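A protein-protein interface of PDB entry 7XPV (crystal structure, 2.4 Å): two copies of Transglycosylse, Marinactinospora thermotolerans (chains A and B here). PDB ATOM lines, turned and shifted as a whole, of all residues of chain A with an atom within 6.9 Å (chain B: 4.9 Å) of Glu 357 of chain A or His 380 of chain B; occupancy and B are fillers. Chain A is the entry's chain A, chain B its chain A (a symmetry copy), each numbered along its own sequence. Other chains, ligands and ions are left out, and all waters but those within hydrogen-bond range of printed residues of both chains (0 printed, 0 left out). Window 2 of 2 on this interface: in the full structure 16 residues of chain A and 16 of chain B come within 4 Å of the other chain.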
ATOM      1  N   HIS A 333      -0.179  10.458 -19.832  1.00  0.00           N
ATOM      2  CA  HIS A 333      -0.636   9.496 -20.827  1.00  0.00           C
ATOM      3  C   HIS A 333      -1.481  10.144 -21.916  1.00  0.00           C
ATOM      4  O   HIS A 333      -1.588   9.583 -23.012  1.00  0.00           O
ATOM      5  CB  HIS A 333      -1.422   8.369 -20.155  1.00  0.00           C
ATOM      6  CG  HIS A 333      -0.563   7.406 -19.396  1.00  0.00           C
ATOM      7  ND1 HIS A 333       0.048   6.324 -19.994  1.00  0.00           N
ATOM      8  CD2 HIS A 333      -0.210   7.363 -18.090  1.00  0.00           C
ATOM      9  CE1 HIS A 333       0.738   5.656 -19.088  1.00  0.00           C
ATOM     10  NE2 HIS A 333       0.599   6.266 -17.924  1.00  0.00           N
ATOM     11  N   HIS A 337      -1.342   9.681 -26.324  1.00  0.00           N
ATOM     12  CA  HIS A 337      -2.514   9.121 -26.992  1.00  0.00           C
ATOM     13  C   HIS A 337      -3.036  10.099 -28.036  1.00  0.00           C
ATOM     14  O   HIS A 337      -3.782  11.030 -27.694  1.00  0.00           O
ATOM     15  CB  HIS A 337      -3.604   8.800 -25.966  1.00  0.00           C
ATOM     16  CG  HIS A 337      -4.099   7.389 -26.031  1.00  0.00           C
ATOM     17  ND1 HIS A 337      -3.618   6.392 -25.211  1.00  0.00           N
ATOM     18  CD2 HIS A 337      -5.032   6.808 -26.823  1.00  0.00           C
ATOM     19  CE1 HIS A 337      -4.235   5.258 -25.490  1.00  0.00           C
ATOM     20  NE2 HIS A 337      -5.097   5.483 -26.466  1.00  0.00           N
ATOM     21  N   SER A 352     -12.850   9.854 -24.717  1.00  0.00           N
ATOM     22  CA  SER A 352     -13.400   8.977 -23.688  1.00  0.00           C
ATOM     23  C   SER A 352     -12.846   7.563 -23.815  1.00  0.00           C
ATOM     24  O   SER A 352     -12.508   6.929 -22.809  1.00  0.00           O
ATOM     25  CB  SER A 352     -14.927   8.968 -23.766  1.00  0.00           C
ATOM     26  OG  SER A 352     -15.376   8.464 -25.012  1.00  0.00           O
ATOM     27  N   TYR A 353     -12.738   7.054 -25.045  1.00  0.00           N
ATOM     28  CA  TYR A 353     -12.147   5.734 -25.238  1.00  0.00           C
ATOM     29  C   TYR A 353     -10.653   5.742 -24.941  1.00  0.00           C
ATOM     30  O   TYR A 353     -10.105   4.724 -24.503  1.00  0.00           O
ATOM     31  CB  TYR A 353     -12.404   5.238 -26.661  1.00  0.00           C
ATOM     32  CG  TYR A 353     -13.851   4.900 -26.941  1.00  0.00           C
ATOM     33  CD1 TYR A 353     -14.459   3.807 -26.335  1.00  0.00           C
ATOM     34  CD2 TYR A 353     -14.606   5.664 -27.822  1.00  0.00           C
ATOM     35  CE1 TYR A 353     -15.781   3.492 -26.591  1.00  0.00           C
ATOM     36  CE2 TYR A 353     -15.929   5.355 -28.085  1.00  0.00           C
ATOM     37  CZ  TYR A 353     -16.512   4.268 -27.467  1.00  0.00           C
ATOM     38  OH  TYR A 353     -17.827   3.954 -27.724  1.00  0.00           O
ATOM     39  N   ALA A 354      -9.981   6.872 -25.171  1.00  0.00           N
ATOM     40  CA  ALA A 354      -8.572   6.975 -24.809  1.00  0.00           C
ATOM     41  C   ALA A 354      -8.379   6.938 -23.298  1.00  0.00           C
ATOM     42  O   ALA A 354      -7.384   6.387 -22.816  1.00  0.00           O
ATOM     43  CB  ALA A 354      -7.968   8.251 -25.394  1.00  0.00           C
ATOM     44  N   LEU A 355      -9.317   7.513 -22.539  1.00  0.00           N
ATOM     45  CA  LEU A 355      -9.223   7.460 -21.084  1.00  0.00           C
ATOM     46  C   LEU A 355      -9.374   6.037 -20.562  1.00  0.00           C
ATOM     47  O   LEU A 355      -8.775   5.687 -19.539  1.00  0.00           O
ATOM     48  CB  LEU A 355     -10.278   8.369 -20.454  1.00  0.00           C
ATOM     49  CG  LEU A 355     -10.132   9.870 -20.704  1.00  0.00           C
ATOM     50  CD1 LEU A 355     -11.345  10.614 -20.177  1.00  0.00           C
ATOM     51  CD2 LEU A 355      -8.859  10.400 -20.064  1.00  0.00           C
ATOM     52  N   GLN A 356     -10.161   5.207 -21.250  1.00  0.00           N
ATOM     53  CA  GLN A 356     -10.334   3.823 -20.823  1.00  0.00           C
ATOM     54  C   GLN A 356      -9.088   2.990 -21.092  1.00  0.00           C
ATOM     55  O   GLN A 356      -8.788   2.065 -20.327  1.00  0.00           O
ATOM     56  CB  GLN A 356     -11.550   3.208 -21.515  1.00  0.00           C
ATOM     57  CG  GLN A 356     -12.879   3.763 -21.027  1.00  0.00           C
ATOM     58  CD  GLN A 356     -14.063   2.959 -21.523  1.00  0.00           C
ATOM     59  OE1 GLN A 356     -14.386   2.975 -22.710  1.00  0.00           O
ATOM     60  NE2 GLN A 356     -14.719   2.250 -20.611  1.00  0.00           N
ATOM     61  N   GLU A 357      -8.356   3.291 -22.167  1.00  0.00           N
ATOM     62  CA  GLU A 357      -7.089   2.608 -22.402  1.00  0.00           C
ATOM     63  C   GLU A 357      -6.022   3.067 -21.420  1.00  0.00           C
ATOM     64  O   GLU A 357      -5.154   2.277 -21.031  1.00  0.00           O
ATOM     65  CB  GLU A 357      -6.621   2.839 -23.840  1.00  0.00           C
ATOM     66  CG  GLU A 357      -7.686   2.587 -24.897  1.00  0.00           C
ATOM     67  CD  GLU A 357      -8.136   1.138 -24.953  1.00  0.00           C
ATOM     68  OE1 GLU A 357      -7.365   0.252 -24.526  1.00  0.00           O
ATOM     69  OE2 GLU A 357      -9.263   0.886 -25.426  1.00  0.00           O
ATOM     70  N   ILE A 358      -6.069   4.336 -21.010  1.00  0.00           N
ATOM     71  CA  ILE A 358      -5.121   4.840 -20.021  1.00  0.00           C
ATOM     72  C   ILE A 358      -5.385   4.211 -18.660  1.00  0.00           C
ATOM     73  O   ILE A 358      -4.451   3.910 -17.907  1.00  0.00           O
ATOM     74  CB  ILE A 358      -5.190   6.377 -19.963  1.00  0.00           C
ATOM     75  CG1 ILE A 358      -4.645   6.985 -21.256  1.00  0.00           C
ATOM     76  CG2 ILE A 358      -4.450   6.909 -18.742  1.00  0.00           C
ATOM     77  CD1 ILE A 358      -4.848   8.480 -21.355  1.00  0.00           C
ATOM     78  N   ALA A 359      -6.661   3.987 -18.329  1.00  0.00           N
ATOM     79  CA  ALA A 359      -7.017   3.425 -17.032  1.00  0.00           C
ATOM     80  C   ALA A 359      -6.418   2.043 -16.808  1.00  0.00           C
ATOM     81  O   ALA A 359      -6.286   1.618 -15.654  1.00  0.00           O
ATOM     82  CB  ALA A 359      -8.538   3.360 -16.889  1.00  0.00           C
ATOM     83  N   GLU A 360      -6.048   1.333 -17.874  1.00  0.00           N
ATOM     84  CA  GLU A 360      -5.475   0.001 -17.746  1.00  0.00           C
ATOM     85  C   GLU A 360      -3.967  -0.036 -17.964  1.00  0.00           C
ATOM     86  O   GLU A 360      -3.312  -0.960 -17.471  1.00  0.00           O
ATOM     87  CB  GLU A 360      -6.148  -0.965 -18.731  1.00  0.00           C
ATOM     88  CG  GLU A 360      -7.662  -1.043 -18.589  1.00  0.00           C
ATOM     89  CD  GLU A 360      -8.104  -1.511 -17.212  1.00  0.00           C
ATOM     90  OE1 GLU A 360      -7.390  -2.334 -16.600  1.00  0.00           O
ATOM     91  OE2 GLU A 360      -9.165  -1.051 -16.742  1.00  0.00           O
ATOM     92  N   ARG A 361      -3.404   0.936 -18.682  1.00  0.00           N
ATOM     93  CA  ARG A 361      -1.964   0.979 -18.900  1.00  0.00           C
ATOM     94  C   ARG A 361      -1.219   1.683 -17.775  1.00  0.00           C
ATOM     95  O   ARG A 361      -0.045   1.379 -17.534  1.00  0.00           O
ATOM     96  CB  ARG A 361      -1.643   1.673 -20.230  1.00  0.00           C
ATOM     97  CG  ARG A 361      -2.163   0.947 -21.464  1.00  0.00           C
ATOM     98  CD  ARG A 361      -1.643   1.570 -22.761  1.00  0.00           C
ATOM     99  NE  ARG A 361      -2.079   2.952 -22.942  1.00  0.00           N
ATOM    100  CZ  ARG A 361      -1.307   4.014 -22.750  1.00  0.00           C
ATOM    101  NH1 ARG A 361      -0.044   3.893 -22.379  1.00  0.00           N
ATOM    102  NH2 ARG A 361      -1.816   5.228 -22.941  1.00  0.00           N
ATOM    103  N   VAL A 362      -1.873   2.615 -17.079  1.00  0.00           N
ATOM    104  CA  VAL A 362      -1.194   3.394 -16.053  1.00  0.00           C
ATOM    105  C   VAL A 362      -0.881   2.511 -14.848  1.00  0.00           C
ATOM    106  O   VAL A 362      -1.617   1.569 -14.523  1.00  0.00           O
ATOM    107  CB  VAL A 362      -2.045   4.613 -15.651  1.00  0.00           C
ATOM    108  CG1 VAL A 362      -3.278   4.183 -14.868  1.00  0.00           C
ATOM    109  CG2 VAL A 362      -1.216   5.612 -14.859  1.00  0.00           C
ATOM    110  N   HIS A 376     -13.305   4.772 -16.258  1.00  0.00           N
ATOM    111  CA  HIS A 376     -14.242   4.041 -17.105  1.00  0.00           C
ATOM    112  C   HIS A 376     -15.655   4.599 -16.982  1.00  0.00           C
ATOM    113  O   HIS A 376     -16.357   4.750 -17.989  1.00  0.00           O
ATOM    114  CB  HIS A 376     -14.219   2.552 -16.758  1.00  0.00           C
ATOM    115  CG  HIS A 376     -12.929   1.873 -17.098  1.00  0.00           C
ATOM    116  ND1 HIS A 376     -12.566   1.571 -18.392  1.00  0.00           N
ATOM    117  CD2 HIS A 376     -11.916   1.438 -16.312  1.00  0.00           C
ATOM    118  CE1 HIS A 376     -11.385   0.979 -18.391  1.00  0.00           C
ATOM    119  NE2 HIS A 376     -10.968   0.885 -17.140  1.00  0.00           N
ATOM    120  N   ARG A 383     -19.749  10.006 -23.030  1.00  0.00           N
ATOM    121  CA  ARG A 383     -20.512   9.593 -24.203  1.00  0.00           C
ATOM    122  C   ARG A 383     -22.003   9.827 -24.008  1.00  0.00           C
ATOM    123  O   ARG A 383     -22.711  10.137 -24.972  1.00  0.00           O
ATOM    124  CB  ARG A 383     -20.244   8.123 -24.516  1.00  0.00           C
ATOM    125  CG  ARG A 383     -18.886   7.856 -25.132  1.00  0.00           C
ATOM    126  CD  ARG A 383     -18.549   6.382 -25.061  1.00  0.00           C
ATOM    127  NE  ARG A 383     -17.366   6.152 -24.244  1.00  0.00           N
ATOM    128  CZ  ARG A 383     -17.015   4.977 -23.740  1.00  0.00           C
ATOM    129  NH1 ARG A 383     -17.754   3.897 -23.927  1.00  0.00           N
ATOM    130  NH2 ARG A 383     -15.896   4.886 -23.031  1.00  0.00           N
ATOM    131  N   HIS B 376     -19.046  -0.624 -15.223  1.00  0.00           N
ATOM    132  CA  HIS B 376     -18.437   0.078 -16.348  1.00  0.00           C
ATOM    133  C   HIS B 376     -17.058  -0.483 -16.673  1.00  0.00           C
ATOM    134  O   HIS B 376     -16.718  -0.666 -17.848  1.00  0.00           O
ATOM    135  CB  HIS B 376     -18.354   1.576 -16.056  1.00  0.00           C
ATOM    136  CG  HIS B 376     -19.688   2.252 -15.979  1.00  0.00           C
ATOM    137  ND1 HIS B 376     -20.451   2.518 -17.095  1.00  0.00           N
ATOM    138  CD2 HIS B 376     -20.394   2.715 -14.920  1.00  0.00           C
ATOM    139  CE1 HIS B 376     -21.571   3.115 -16.728  1.00  0.00           C
ATOM    140  NE2 HIS B 376     -21.561   3.247 -15.414  1.00  0.00           N
ATOM    141  N   ARG B 377     -16.249  -0.765 -15.651  1.00  0.00           N
ATOM    142  CA  ARG B 377     -14.923  -1.319 -15.909  1.00  0.00           C
ATOM    143  C   ARG B 377     -15.013  -2.762 -16.388  1.00  0.00           C
ATOM    144  O   ARG B 377     -14.243  -3.178 -17.262  1.00  0.00           O
ATOM    145  CB  ARG B 377     -14.052  -1.213 -14.657  1.00  0.00           C
ATOM    146  CG  ARG B 377     -12.624  -1.696 -14.863  1.00  0.00           C
ATOM    147  CD  ARG B 377     -11.698  -1.170 -13.779  1.00  0.00           C
ATOM    148  NE  ARG B 377     -10.316  -1.580 -14.001  1.00  0.00           N
ATOM    149  CZ  ARG B 377      -9.722  -2.584 -13.372  1.00  0.00           C
ATOM    150  NH1 ARG B 377     -10.355  -3.297 -12.454  1.00  0.00           N
ATOM    151  NH2 ARG B 377      -8.459  -2.878 -13.668  1.00  0.00           N
ATOM    152  N   SER B 378     -15.950  -3.539 -15.836  1.00  0.00           N
ATOM    153  CA  SER B 378     -16.139  -4.911 -16.302  1.00  0.00           C
ATOM    154  C   SER B 378     -16.548  -4.941 -17.767  1.00  0.00           C
ATOM    155  O   SER B 378     -16.108  -5.814 -18.525  1.00  0.00           O
ATOM    156  CB  SER B 378     -17.188  -5.623 -15.446  1.00  0.00           C
ATOM    157  OG  SER B 378     -16.798  -5.683 -14.087  1.00  0.00           O
ATOM    158  N   ALA B 379     -17.391  -3.992 -18.185  1.00  0.00           N
ATOM    159  CA  ALA B 379     -17.826  -3.941 -19.576  1.00  0.00           C
ATOM    160  C   ALA B 379     -16.661  -3.645 -20.511  1.00  0.00           C
ATOM    161  O   ALA B 379     -16.581  -4.209 -21.608  1.00  0.00           O
ATOM    162  CB  ALA B 379     -18.926  -2.893 -19.740  1.00  0.00           C
ATOM    163  N   HIS B 380     -15.750  -2.760 -20.097  1.00  0.00           N
ATOM    164  CA  HIS B 380     -14.560  -2.497 -20.900  1.00  0.00           C
ATOM    165  C   HIS B 380     -13.668  -3.729 -20.985  1.00  0.00           C
ATOM    166  O   HIS B 380     -13.088  -4.009 -22.039  1.00  0.00           O
ATOM    167  CB  HIS B 380     -13.786  -1.312 -20.322  1.00  0.00           C
ATOM    168  CG  HIS B 380     -12.431  -1.121 -20.929  1.00  0.00           C
ATOM    169  ND1 HIS B 380     -12.233  -0.439 -22.109  1.00  0.00           N
ATOM    170  CD2 HIS B 380     -11.205  -1.530 -20.521  1.00  0.00           C
ATOM    171  CE1 HIS B 380     -10.944  -0.430 -22.400  1.00  0.00           C
ATOM    172  NE2 HIS B 380     -10.299  -1.086 -21.452  1.00  0.00           N
ATOM    173  N   LEU B 381     -13.545  -4.475 -19.884  1.00  0.00           N
ATOM    174  CA  LEU B 381     -12.743  -5.694 -19.905  1.00  0.00           C
ATOM    175  C   LEU B 381     -13.404  -6.783 -20.740  1.00  0.00           C
ATOM    176  O   LEU B 381     -12.711  -7.655 -21.277  1.00  0.00           O
ATOM    177  CB  LEU B 381     -12.501  -6.187 -18.478  1.00  0.00           C
ATOM    178  CG  LEU B 381     -11.720  -5.237 -17.566  1.00  0.00           C
ATOM    179  CD1 LEU B 381     -11.669  -5.771 -16.144  1.00  0.00           C
ATOM    180  CD2 LEU B 381     -10.316  -5.008 -18.108  1.00  0.00           C
ATOM    181  N   MET B 382     -14.733  -6.749 -20.858  1.00  0.00           N
ATOM    182  CA  MET B 382     -15.426  -7.684 -21.738  1.00  0.00           C
ATOM    183  C   MET B 382     -15.150  -7.369 -23.203  1.00  0.00           C
ATOM    184  O   MET B 382     -14.967  -8.284 -24.017  1.00  0.00           O
ATOM    185  CB  MET B 382     -16.929  -7.652 -21.454  1.00  0.00           C
ATOM    186  CG  MET B 382     -17.312  -8.241 -20.104  1.00  0.00           C
ATOM    187  SD  MET B 382     -18.948  -7.737 -19.536  1.00  0.00           S
ATOM    188  CE  MET B 382     -19.987  -8.449 -20.810  1.00  0.00           C
ATOM    189  N   ARG B 383     -15.116  -6.082 -23.562  1.00  0.00           N
ATOM    190  CA  ARG B 383     -14.776  -5.707 -24.930  1.00  0.00           C
ATOM    191  C   ARG B 383     -13.301  -5.942 -25.221  1.00  0.00           C
ATOM    192  O   ARG B 383     -12.941  -6.284 -26.354  1.00  0.00           O
ATOM    193  CB  ARG B 383     -15.137  -4.246 -25.182  1.00  0.00           C
ATOM    194  CG  ARG B 383     -16.623  -3.990 -25.332  1.00  0.00           C
ATOM    195  CD  ARG B 383     -16.926  -2.513 -25.199  1.00  0.00           C
ATOM    196  NE  ARG B 383     -17.782  -2.254 -24.050  1.00  0.00           N
ATOM    197  CZ  ARG B 383     -17.956  -1.063 -23.494  1.00  0.00           C
ATOM    198  NH1 ARG B 383     -17.323   0.008 -23.941  1.00  0.00           N
ATOM    199  NH2 ARG B 383     -18.786  -0.946 -22.464  1.00  0.00           N
ATOM    200  N   SER B 384     -12.437  -5.751 -24.222  1.00  0.00           N
ATOM    201  CA  SER B 384     -11.027  -6.087 -24.387  1.00  0.00           C
ATOM    202  C   SER B 384     -10.836  -7.586 -24.573  1.00  0.00           C
ATOM    203  O   SER B 384      -9.896  -8.012 -25.252  1.00  0.00           O
ATOM    204  CB  SER B 384     -10.230  -5.583 -23.181  1.00  0.00           C
ATOM    205  OG  SER B 384      -8.844  -5.833 -23.335  1.00  0.00           O
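OE2 of Glu 360 of chain A is in salt-bridge range of NE of Arg 377 of chain B (3.0 Å).
OG of Ser 352 of chain A lies within hydrogen-bond range of NE of Arg 383 of chain A, 3.1 Å away.
The side-chain amide nitrogen of Gln 356 of chain A lies within hydrogen-bond range of a ring nitrogen (ND1) of His 376 of chain A, 3.2 Å away.
The guanidinium group of Arg 383 of chain A sits at hydrogen-bond distance from the side-chain amide oxygen of Gln 356 of chain A (2.5 Å).
The side-chain carboxylate of Glu 360 of chain A lies within hydrogen-bond range of a ring nitrogen (NE2) of His 376 of chain A (2.7 Å).
The guanidinium group (NE) of Arg 383 of chain B is in hydrogen-bond range of the backbone carbonyl oxygen (O) of Ala 379 of chain B (3.4 Å).
Among the printed residues, merely in contact across the chains: His 376 of chain A with His 380 of chain B (3.3 Å), His 376 of chain A with Arg 377 of chain B (3.5 Å), Gln 356 of chain A with His 380 of chain B (3.7 Å), Glu 357 of chain A with His 380 of chain B (3.7 Å), Glu 360 of chain A with His 380 of chain B (3.9 Å) and Arg 383 of chain A with Arg 383 of chain B (3.9 Å).
Of the printed residues of chain B, Gln 356 of chain A touches His 380 (3.7 Å).
Of the printed residues of chain B, Glu 357 of chain A touches His 380.
Of the printed residues of chain B, His 376 of chain A touches Arg 377 (3.5 Å) and His 380 (3.3 Å).
Printed residues of chain B within 4 Å of Arg 383 of chain A: Arg 383 (3.9 Å).
Of the printed residues of chain A, Arg 377 of chain B touches Glu 360 and His 376.
Of chain A, only Gln 356 (3.7 Å), Glu 357 (3.7 Å), Glu 360 (3.9 Å) and His 376 (3.3 Å) come within 4 Å of His 380 of chain B.
Of the printed residues of chain A, Arg 383 of chain B touches Arg 383 (3.9 Å).
The nearest printed residue of chain B that does not touch Glu 357 of chain A is Ser 384 of chain B (6.4 Å).
The nearest residue of chain A that does not touch His 380 of chain B is Tyr 353 of chain A (5.6 Å).
Of the 15 printed residues of chain A, 5 touch a printed residue of chain B.
Printed residues of chain B that touch a printed residue of chain A: Arg 377, His 380 and Arg 383.
Hydrophobic or aromatic side chains of chain B within 4 Å of the printed part of chain A: His 380.
Along chain B the printed residues that touch a printed residue of chain A span positions 377 to 383.
Among the printed residues, Asp or Glu carboxylates within 4 Å of a Lys or Arg side-chain nitrogen of the other chain: Glu 360 of chain A with Arg 377 of chain B (3.0 Å).
Arg 383 of chain B touches its own counterpart, Arg 383 of chain A.
Positions printed for both chains: 376 and 383.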
